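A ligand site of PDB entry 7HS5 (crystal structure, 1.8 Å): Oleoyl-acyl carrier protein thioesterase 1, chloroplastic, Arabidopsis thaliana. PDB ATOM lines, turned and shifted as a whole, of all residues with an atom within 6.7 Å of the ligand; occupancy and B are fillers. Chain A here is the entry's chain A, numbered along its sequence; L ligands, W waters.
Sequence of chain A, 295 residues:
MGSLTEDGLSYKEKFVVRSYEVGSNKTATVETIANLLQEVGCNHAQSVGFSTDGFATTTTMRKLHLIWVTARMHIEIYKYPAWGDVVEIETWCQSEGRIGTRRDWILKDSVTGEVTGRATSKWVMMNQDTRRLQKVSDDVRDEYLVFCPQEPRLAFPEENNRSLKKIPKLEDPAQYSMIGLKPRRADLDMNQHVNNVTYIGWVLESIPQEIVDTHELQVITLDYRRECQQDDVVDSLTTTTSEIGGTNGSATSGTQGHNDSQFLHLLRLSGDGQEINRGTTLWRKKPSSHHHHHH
The indole nitrogen (NE1) of Trp 68 lies within hydrogen-bond range of the side-chain sulfur (SD) of Met 61, at 3.5 Å. The guanidinium group (NH2) of Arg 103 lies within hydrogen-bond range of a ring nitrogen (ND1) of His 44 (2.9 Å). SG of Cys 93 is in hydrogen-bond range of NH1 of Arg 103. O of Ala 45 lies within hydrogen-bond range of N of Phe 50 (3.0 Å). The backbone carbonyl oxygen (O) of His 44 sits at hydrogen-bond distance from the side-chain hydroxyl (OG) of Ser 47. The backbone carbonyl oxygen of Tyr 144 sits at hydrogen-bond distance from the side-chain sulfur of Cys 148 (3.6 Å). The backbone carbonyl oxygen (O) of Cys 93 lies close to the side-chain sulfur (SG) of Cys 148 (3.4 Å).
The indole nitrogen (NE1) of Trp 68 sits at hydrogen-bond distance from a nitrogen (N1) of the ligand, at 2.9 Å. NH1 of Arg 103 lies within hydrogen-bond range of N3 of the ligand.
NE2 of His 44 touches C1 of the ligand, at 3.5 Å. Ala 45 touches the ligand. Val 48 touches the ligand. Phe 50 touches the ligand (CD2 to C2, 3.6 Å). Ala 56 touches the ligand. SG of Cys 93 touches C6 of the ligand, at 3.9 Å. CG2 of Thr 101 touches C4 of the ligand, 3.6 Å away. Tyr 144 touches the ligand. CB of Phe 147 touches C8 of the ligand, 3.7 Å away. Of the 23 residues printed, 11 come within 4 Å of the ligand. The nearest printed residue that does not touch the ligand is Cys 148 (4.3 Å).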
ATOM      1  N   GLY A  41     -24.995 -26.918  17.865  1.00  0.00           N
ATOM      2  CA  GLY A  41     -25.868 -25.795  17.526  1.00  0.00           C
ATOM      3  C   GLY A  41     -25.166 -24.462  17.761  1.00  0.00           C
ATOM      4  O   GLY A  41     -25.230 -23.561  16.900  1.00  0.00           O
ATOM      5  N   HIS A  44     -22.310 -23.921  15.213  1.00  0.00           N
ATOM      6  CA  HIS A  44     -22.875 -23.554  13.939  1.00  0.00           C
ATOM      7  C   HIS A  44     -23.162 -22.024  13.937  1.00  0.00           C
ATOM      8  O   HIS A  44     -22.700 -21.321  13.026  1.00  0.00           O
ATOM      9  CB  HIS A  44     -24.140 -24.394  13.647  1.00  0.00           C
ATOM     10  CG  HIS A  44     -24.803 -24.080  12.333  1.00  0.00           C
ATOM     11  ND1 HIS A  44     -26.123 -24.447  12.089  1.00  0.00           N
ATOM     12  CD2 HIS A  44     -24.328 -23.433  11.246  1.00  0.00           C
ATOM     13  CE1 HIS A  44     -26.381 -24.030  10.851  1.00  0.00           C
ATOM     14  NE2 HIS A  44     -25.346 -23.378  10.329  1.00  0.00           N
ATOM     15  N   ALA A  45     -23.870 -21.521  14.958  1.00  0.00           N
ATOM     16  CA  ALA A  45     -24.185 -20.090  15.114  1.00  0.00           C
ATOM     17  C   ALA A  45     -22.910 -19.226  15.110  1.00  0.00           C
ATOM     18  O   ALA A  45     -22.853 -18.234  14.387  1.00  0.00           O
ATOM     19  CB  ALA A  45     -24.984 -19.851  16.382  1.00  0.00           C
ATOM     20  N   GLN A  46     -21.875 -19.636  15.839  1.00  0.00           N
ATOM     21  CA  GLN A  46     -20.611 -18.911  15.892  1.00  0.00           C
ATOM     22  C   GLN A  46     -19.886 -18.845  14.549  1.00  0.00           C
ATOM     23  O   GLN A  46     -19.317 -17.801  14.213  1.00  0.00           O
ATOM     24  CB  GLN A  46     -19.656 -19.547  16.920  1.00  0.00           C
ATOM     25  CG  GLN A  46     -19.954 -19.199  18.369  1.00  0.00           C
ATOM     26  CD  GLN A  46     -19.110 -20.045  19.304  1.00  0.00           C
ATOM     27  OE1 GLN A  46     -19.481 -21.168  19.680  1.00  0.00           O
ATOM     28  NE2 GLN A  46     -17.959 -19.521  19.728  1.00  0.00           N
ATOM     29  N   SER A  47     -19.910 -19.947  13.790  1.00  0.00           N
ATOM     30  CA  SER A  47     -19.235 -20.053  12.503  1.00  0.00           C
ATOM     31  C   SER A  47     -19.787 -19.128  11.417  1.00  0.00           C
ATOM     32  O   SER A  47     -19.079 -18.850  10.447  1.00  0.00           O
ATOM     33  CB  SER A  47     -19.237 -21.501  12.007  1.00  0.00           C
ATOM     34  OG  SER A  47     -20.528 -21.891  11.569  1.00  0.00           O
ATOM     35  N   VAL A  48     -21.024 -18.671  11.552  1.00  0.00           N
ATOM     36  CA  VAL A  48     -21.633 -17.783  10.550  1.00  0.00           C
ATOM     37  C   VAL A  48     -21.874 -16.343  11.058  1.00  0.00           C
ATOM     38  O   VAL A  48     -22.595 -15.593  10.396  1.00  0.00           O
ATOM     39  CB  VAL A  48     -22.904 -18.378   9.924  1.00  0.00           C
ATOM     40  CG1 VAL A  48     -22.571 -19.627   9.120  1.00  0.00           C
ATOM     41  CG2 VAL A  48     -23.967 -18.671  10.981  1.00  0.00           C
ATOM     42  N   PHE A  50     -23.061 -15.278  14.342  1.00  0.00           N
ATOM     43  CA  PHE A  50     -23.956 -15.024  15.476  1.00  0.00           C
ATOM     44  C   PHE A  50     -23.191 -15.287  16.777  1.00  0.00           C
ATOM     45  O   PHE A  50     -22.478 -16.276  16.858  1.00  0.00           O
ATOM     46  CB  PHE A  50     -25.259 -15.820  15.342  1.00  0.00           C
ATOM     47  CG  PHE A  50     -25.969 -15.539  14.038  1.00  0.00           C
ATOM     48  CD1 PHE A  50     -26.497 -14.289  13.769  1.00  0.00           C
ATOM     49  CD2 PHE A  50     -26.097 -16.529  13.076  1.00  0.00           C
ATOM     50  CE1 PHE A  50     -27.156 -14.043  12.574  1.00  0.00           C
ATOM     51  CE2 PHE A  50     -26.754 -16.269  11.880  1.00  0.00           C
ATOM     52  CZ  PHE A  50     -27.272 -15.026  11.630  1.00  0.00           C
ATOM     53  N   ALA A  56     -27.628 -16.782  20.365  1.00  0.00           N
ATOM     54  CA  ALA A  56     -27.581 -16.750  18.902  1.00  0.00           C
ATOM     55  C   ALA A  56     -28.663 -15.769  18.466  1.00  0.00           C
ATOM     56  O   ALA A  56     -29.837 -16.129  18.423  1.00  0.00           O
ATOM     57  CB  ALA A  56     -27.866 -18.136  18.344  1.00  0.00           C
ATOM     58  N   THR A  57     -28.285 -14.515  18.195  1.00  0.00           N
ATOM     59  CA  THR A  57     -29.225 -13.460  17.825  1.00  0.00           C
ATOM     60  C   THR A  57     -28.782 -12.704  16.576  1.00  0.00           C
ATOM     61  O   THR A  57     -27.586 -12.516  16.366  1.00  0.00           O
ATOM     62  CB  THR A  57     -29.311 -12.411  18.955  1.00  0.00           C
ATOM     63  OG1 THR A  57     -28.022 -11.845  19.178  1.00  0.00           O
ATOM     64  CG2 THR A  57     -29.841 -12.991  20.267  1.00  0.00           C
ATOM     65  N   THR A  58     -29.752 -12.200  15.801  1.00  0.00           N
ATOM     66  CA  THR A  58     -29.422 -11.357  14.645  1.00  0.00           C
ATOM     67  C   THR A  58     -29.166  -9.893  15.146  1.00  0.00           C
ATOM     68  O   THR A  58     -29.279  -9.633  16.350  1.00  0.00           O
ATOM     69  CB  THR A  58     -30.521 -11.467  13.537  1.00  0.00           C
ATOM     70  OG1 THR A  58     -31.627 -10.621  13.870  1.00  0.00           O
ATOM     71  CG2 THR A  58     -31.000 -12.896  13.310  1.00  0.00           C
ATOM     72  N   MET A  61     -32.412  -8.387  16.488  1.00  0.00           N
ATOM     73  CA  MET A  61     -32.758  -9.027  17.763  1.00  0.00           C
ATOM     74  C   MET A  61     -32.021  -8.358  18.935  1.00  0.00           C
ATOM     75  O   MET A  61     -32.619  -8.115  19.973  1.00  0.00           O
ATOM     76  CB  MET A  61     -32.442 -10.532  17.731  1.00  0.00           C
ATOM     77  CG  MET A  61     -33.370 -11.352  16.854  1.00  0.00           C
ATOM     78  SD  MET A  61     -32.936 -13.118  16.811  1.00  0.00           S
ATOM     79  CE  MET A  61     -33.171 -13.530  18.479  1.00  0.00           C
ATOM     80  N   TRP A  68     -34.076 -16.169  21.175  1.00  0.00           N
ATOM     81  CA  TRP A  68     -34.753 -17.395  20.770  1.00  0.00           C
ATOM     82  C   TRP A  68     -34.821 -18.277  22.015  1.00  0.00           C
ATOM     83  O   TRP A  68     -33.815 -18.410  22.708  1.00  0.00           O
ATOM     84  CB  TRP A  68     -33.919 -18.140  19.697  1.00  0.00           C
ATOM     85  CG  TRP A  68     -33.970 -17.540  18.321  1.00  0.00           C
ATOM     86  CD1 TRP A  68     -32.933 -17.014  17.619  1.00  0.00           C
ATOM     87  CD2 TRP A  68     -35.116 -17.491  17.465  1.00  0.00           C
ATOM     88  NE1 TRP A  68     -33.367 -16.610  16.376  1.00  0.00           N
ATOM     89  CE2 TRP A  68     -34.703 -16.895  16.249  1.00  0.00           C
ATOM     90  CE3 TRP A  68     -36.455 -17.872  17.608  1.00  0.00           C
ATOM     91  CZ2 TRP A  68     -35.577 -16.675  15.190  1.00  0.00           C
ATOM     92  CZ3 TRP A  68     -37.322 -17.653  16.556  1.00  0.00           C
ATOM     93  CH2 TRP A  68     -36.874 -17.079  15.360  1.00  0.00           C
ATOM     94  N   TRP A  92     -28.595 -27.968  11.161  1.00  0.00           N
ATOM     95  CA  TRP A  92     -29.027 -26.892  10.298  1.00  0.00           C
ATOM     96  C   TRP A  92     -30.282 -26.242  10.871  1.00  0.00           C
ATOM     97  O   TRP A  92     -30.983 -26.831  11.696  1.00  0.00           O
ATOM     98  CB  TRP A  92     -29.280 -27.376   8.839  1.00  0.00           C
ATOM     99  CG  TRP A  92     -30.461 -28.299   8.695  1.00  0.00           C
ATOM    100  CD1 TRP A  92     -31.735 -27.942   8.352  1.00  0.00           C
ATOM    101  CD2 TRP A  92     -30.461 -29.718   8.830  1.00  0.00           C
ATOM    102  NE1 TRP A  92     -32.535 -29.059   8.304  1.00  0.00           N
ATOM    103  CE2 TRP A  92     -31.776 -30.171   8.578  1.00  0.00           C
ATOM    104  CE3 TRP A  92     -29.461 -30.666   9.114  1.00  0.00           C
ATOM    105  CZ2 TRP A  92     -32.126 -31.519   8.623  1.00  0.00           C
ATOM    106  CZ3 TRP A  92     -29.813 -32.008   9.129  1.00  0.00           C
ATOM    107  CH2 TRP A  92     -31.125 -32.423   8.922  1.00  0.00           C
ATOM    108  N   CYS A  93     -30.544 -25.012  10.418  1.00  0.00           N
ATOM    109  CA  CYS A  93     -31.692 -24.212  10.802  1.00  0.00           C
ATOM    110  C   CYS A  93     -32.609 -24.022   9.637  1.00  0.00           C
ATOM    111  O   CYS A  93     -32.169 -23.934   8.500  1.00  0.00           O
ATOM    112  CB  CYS A  93     -31.235 -22.863  11.338  1.00  0.00           C
ATOM    113  SG  CYS A  93     -30.567 -22.910  13.001  1.00  0.00           S
ATOM    114  N   GLN A  94     -33.884 -23.863   9.921  1.00  0.00           N
ATOM    115  CA  GLN A  94     -34.872 -23.565   8.909  1.00  0.00           C
ATOM    116  C   GLN A  94     -35.874 -22.582   9.435  1.00  0.00           C
ATOM    117  O   GLN A  94     -36.295 -22.663  10.596  1.00  0.00           O
ATOM    118  CB  GLN A  94     -35.553 -24.837   8.413  1.00  0.00           C
ATOM    119  CG  GLN A  94     -34.836 -25.452   7.235  1.00  0.00           C
ATOM    120  CD  GLN A  94     -35.825 -25.829   6.174  1.00  0.00           C
ATOM    121  OE1 GLN A  94     -36.642 -26.745   6.344  1.00  0.00           O
ATOM    122  NE2 GLN A  94     -35.778 -25.118   5.061  1.00  0.00           N
ATOM    123  N   THR A 101     -38.365 -20.459  14.391  1.00  0.00           N
ATOM    124  CA  THR A 101     -37.367 -21.229  13.654  1.00  0.00           C
ATOM    125  C   THR A 101     -37.350 -22.671  14.179  1.00  0.00           C
ATOM    126  O   THR A 101     -37.898 -22.975  15.253  1.00  0.00           O
ATOM    127  CB  THR A 101     -35.948 -20.609  13.768  1.00  0.00           C
ATOM    128  OG1 THR A 101     -35.652 -20.293  15.137  1.00  0.00           O
ATOM    129  CG2 THR A 101     -35.746 -19.432  12.857  1.00  0.00           C
ATOM    130  N   ARG A 102     -36.688 -23.544  13.441  1.00  0.00           N
ATOM    131  CA  ARG A 102     -36.503 -24.938  13.761  1.00  0.00           C
ATOM    132  C   ARG A 102     -35.005 -25.266  13.627  1.00  0.00           C
ATOM    133  O   ARG A 102     -34.351 -24.793  12.681  1.00  0.00           O
ATOM    134  CB  ARG A 102     -37.328 -25.760  12.757  1.00  0.00           C
ATOM    135  CG  ARG A 102     -37.626 -27.183  13.179  1.00  0.00           C
ATOM    136  CD  ARG A 102     -38.353 -27.956  12.087  1.00  0.00           C
ATOM    137  NE  ARG A 102     -37.410 -28.470  11.094  1.00  0.00           N
ATOM    138  CZ  ARG A 102     -37.305 -28.029   9.839  1.00  0.00           C
ATOM    139  NH1 ARG A 102     -36.396 -28.542   9.029  1.00  0.00           N
ATOM    140  NH2 ARG A 102     -38.122 -27.083   9.394  1.00  0.00           N
ATOM    141  N   ARG A 103     -34.432 -25.991  14.597  1.00  0.00           N
ATOM    142  CA  ARG A 103     -33.068 -26.475  14.448  1.00  0.00           C
ATOM    143  C   ARG A 103     -33.175 -27.979  14.428  1.00  0.00           C
ATOM    144  O   ARG A 103     -33.786 -28.548  15.334  1.00  0.00           O
ATOM    145  CB  ARG A 103     -32.079 -25.978  15.527  1.00  0.00           C
ATOM    146  CG  ARG A 103     -30.709 -26.675  15.381  1.00  0.00           C
ATOM    147  CD  ARG A 103     -29.626 -26.145  16.298  1.00  0.00           C
ATOM    148  NE  ARG A 103     -29.214 -24.781  15.973  1.00  0.00           N
ATOM    149  CZ  ARG A 103     -28.352 -24.461  15.006  1.00  0.00           C
ATOM    150  NH1 ARG A 103     -28.015 -23.196  14.802  1.00  0.00           N
ATOM    151  NH2 ARG A 103     -27.851 -25.406  14.225  1.00  0.00           N
ATOM    152  N   VAL A 140     -36.051  -9.340  10.878  1.00  0.00           N
ATOM    153  CA  VAL A 140     -35.279 -10.391  11.533  1.00  0.00           C
ATOM    154  C   VAL A 140     -35.171 -11.610  10.625  1.00  0.00           C
ATOM    155  O   VAL A 140     -34.069 -12.085  10.371  1.00  0.00           O
ATOM    156  CB  VAL A 140     -35.832 -10.747  12.927  1.00  0.00           C
ATOM    157  CG1 VAL A 140     -35.136 -11.966  13.513  1.00  0.00           C
ATOM    158  CG2 VAL A 140     -35.707  -9.566  13.881  1.00  0.00           C
ATOM    159  N   TYR A 144     -31.428 -13.826   8.735  1.00  0.00           N
ATOM    160  CA  TYR A 144     -30.889 -15.170   8.956  1.00  0.00           C
ATOM    161  C   TYR A 144     -31.208 -16.177   7.849  1.00  0.00           C
ATOM    162  O   TYR A 144     -30.624 -17.262   7.849  1.00  0.00           O
ATOM    163  CB  TYR A 144     -31.303 -15.732  10.333  1.00  0.00           C
ATOM    164  CG  TYR A 144     -32.790 -15.970  10.519  1.00  0.00           C
ATOM    165  CD1 TYR A 144     -33.426 -17.043   9.908  1.00  0.00           C
ATOM    166  CD2 TYR A 144     -33.520 -15.195  11.401  1.00  0.00           C
ATOM    167  CE1 TYR A 144     -34.777 -17.281  10.085  1.00  0.00           C
ATOM    168  CE2 TYR A 144     -34.869 -15.438  11.607  1.00  0.00           C
ATOM    169  CZ  TYR A 144     -35.507 -16.471  10.937  1.00  0.00           C
ATOM    170  OH  TYR A 144     -36.844 -16.708  11.144  1.00  0.00           O
ATOM    171  N   LEU A 145     -32.136 -15.850   6.939  1.00  0.00           N
ATOM    172  CA  LEU A 145     -32.556 -16.758   5.879  1.00  0.00           C
ATOM    173  C   LEU A 145     -31.429 -17.236   4.961  1.00  0.00           C
ATOM    174  O   LEU A 145     -31.420 -18.390   4.571  1.00  0.00           O
ATOM    175  CB  LEU A 145     -33.713 -16.182   5.066  1.00  0.00           C
ATOM    176  CG  LEU A 145     -34.993 -17.023   5.109  1.00  0.00           C
ATOM    177  CD1 LEU A 145     -36.244 -16.140   5.083  1.00  0.00           C
ATOM    178  CD2 LEU A 145     -34.995 -18.089   3.991  1.00  0.00           C
ATOM    179  N   PHE A 147     -28.588 -18.124   5.745  1.00  0.00           N
ATOM    180  CA  PHE A 147     -27.809 -19.145   6.439  1.00  0.00           C
ATOM    181  C   PHE A 147     -28.575 -20.483   6.582  1.00  0.00           C
ATOM    182  O   PHE A 147     -28.051 -21.431   7.164  1.00  0.00           O
ATOM    183  CB  PHE A 147     -27.343 -18.604   7.811  1.00  0.00           C
ATOM    184  CG  PHE A 147     -26.597 -17.292   7.708  1.00  0.00           C
ATOM    185  CD1 PHE A 147     -25.296 -17.253   7.240  1.00  0.00           C
ATOM    186  CD2 PHE A 147     -27.228 -16.095   8.008  1.00  0.00           C
ATOM    187  CE1 PHE A 147     -24.618 -16.037   7.107  1.00  0.00           C
ATOM    188  CE2 PHE A 147     -26.562 -14.887   7.857  1.00  0.00           C
ATOM    189  CZ  PHE A 147     -25.267 -14.868   7.395  1.00  0.00           C
ATOM    190  N   CYS A 148     -29.799 -20.575   6.039  1.00  0.00           N
ATOM    191  CA  CYS A 148     -30.698 -21.711   6.096  1.00  0.00           C
ATOM    192  C   CYS A 148     -30.940 -22.313   4.700  1.00  0.00           C
ATOM    193  O   CYS A 148     -30.958 -21.567   3.715  1.00  0.00           O
ATOM    194  CB  CYS A 148     -32.022 -21.269   6.701  1.00  0.00           C
ATOM    195  SG  CYS A 148     -31.889 -20.573   8.374  1.00  0.00           S
HETATM  196  C1  LIG L   1     -26.925 -20.734  11.969  1.00  0.00           C
HETATM  197  C2  LIG L   1     -29.340 -16.844  14.650  1.00  0.00           C
HETATM  198  C3  LIG L   1     -30.464 -17.533  13.968  1.00  0.00           C
HETATM  199  N1  LIG L   1     -31.734 -17.197  14.077  1.00  0.00           N
HETATM  200  C4  LIG L   1     -32.432 -18.117  13.294  1.00  0.00           C
HETATM  201  C5  LIG L   1     -31.586 -18.993  12.725  1.00  0.00           C
HETATM  202  N2  LIG L   1     -30.319 -18.652  13.175  1.00  0.00           N
HETATM  203  C6  LIG L   1     -29.111 -19.316  12.738  1.00  0.00           C
HETATM  204  C7  LIG L   1     -28.941 -19.611  11.400  1.00  0.00           C
HETATM  205  C8  LIG L   1     -27.813 -20.312  11.012  1.00  0.00           C
HETATM  206  N3  LIG L   1     -27.108 -20.517  13.274  1.00  0.00           N
HETATM  207  C9  LIG L   1     -28.193 -19.840  13.655  1.00  0.00           C
HETATM  208  O   HOH W   1     -28.871 -21.273  16.738  1.00  0.00           O
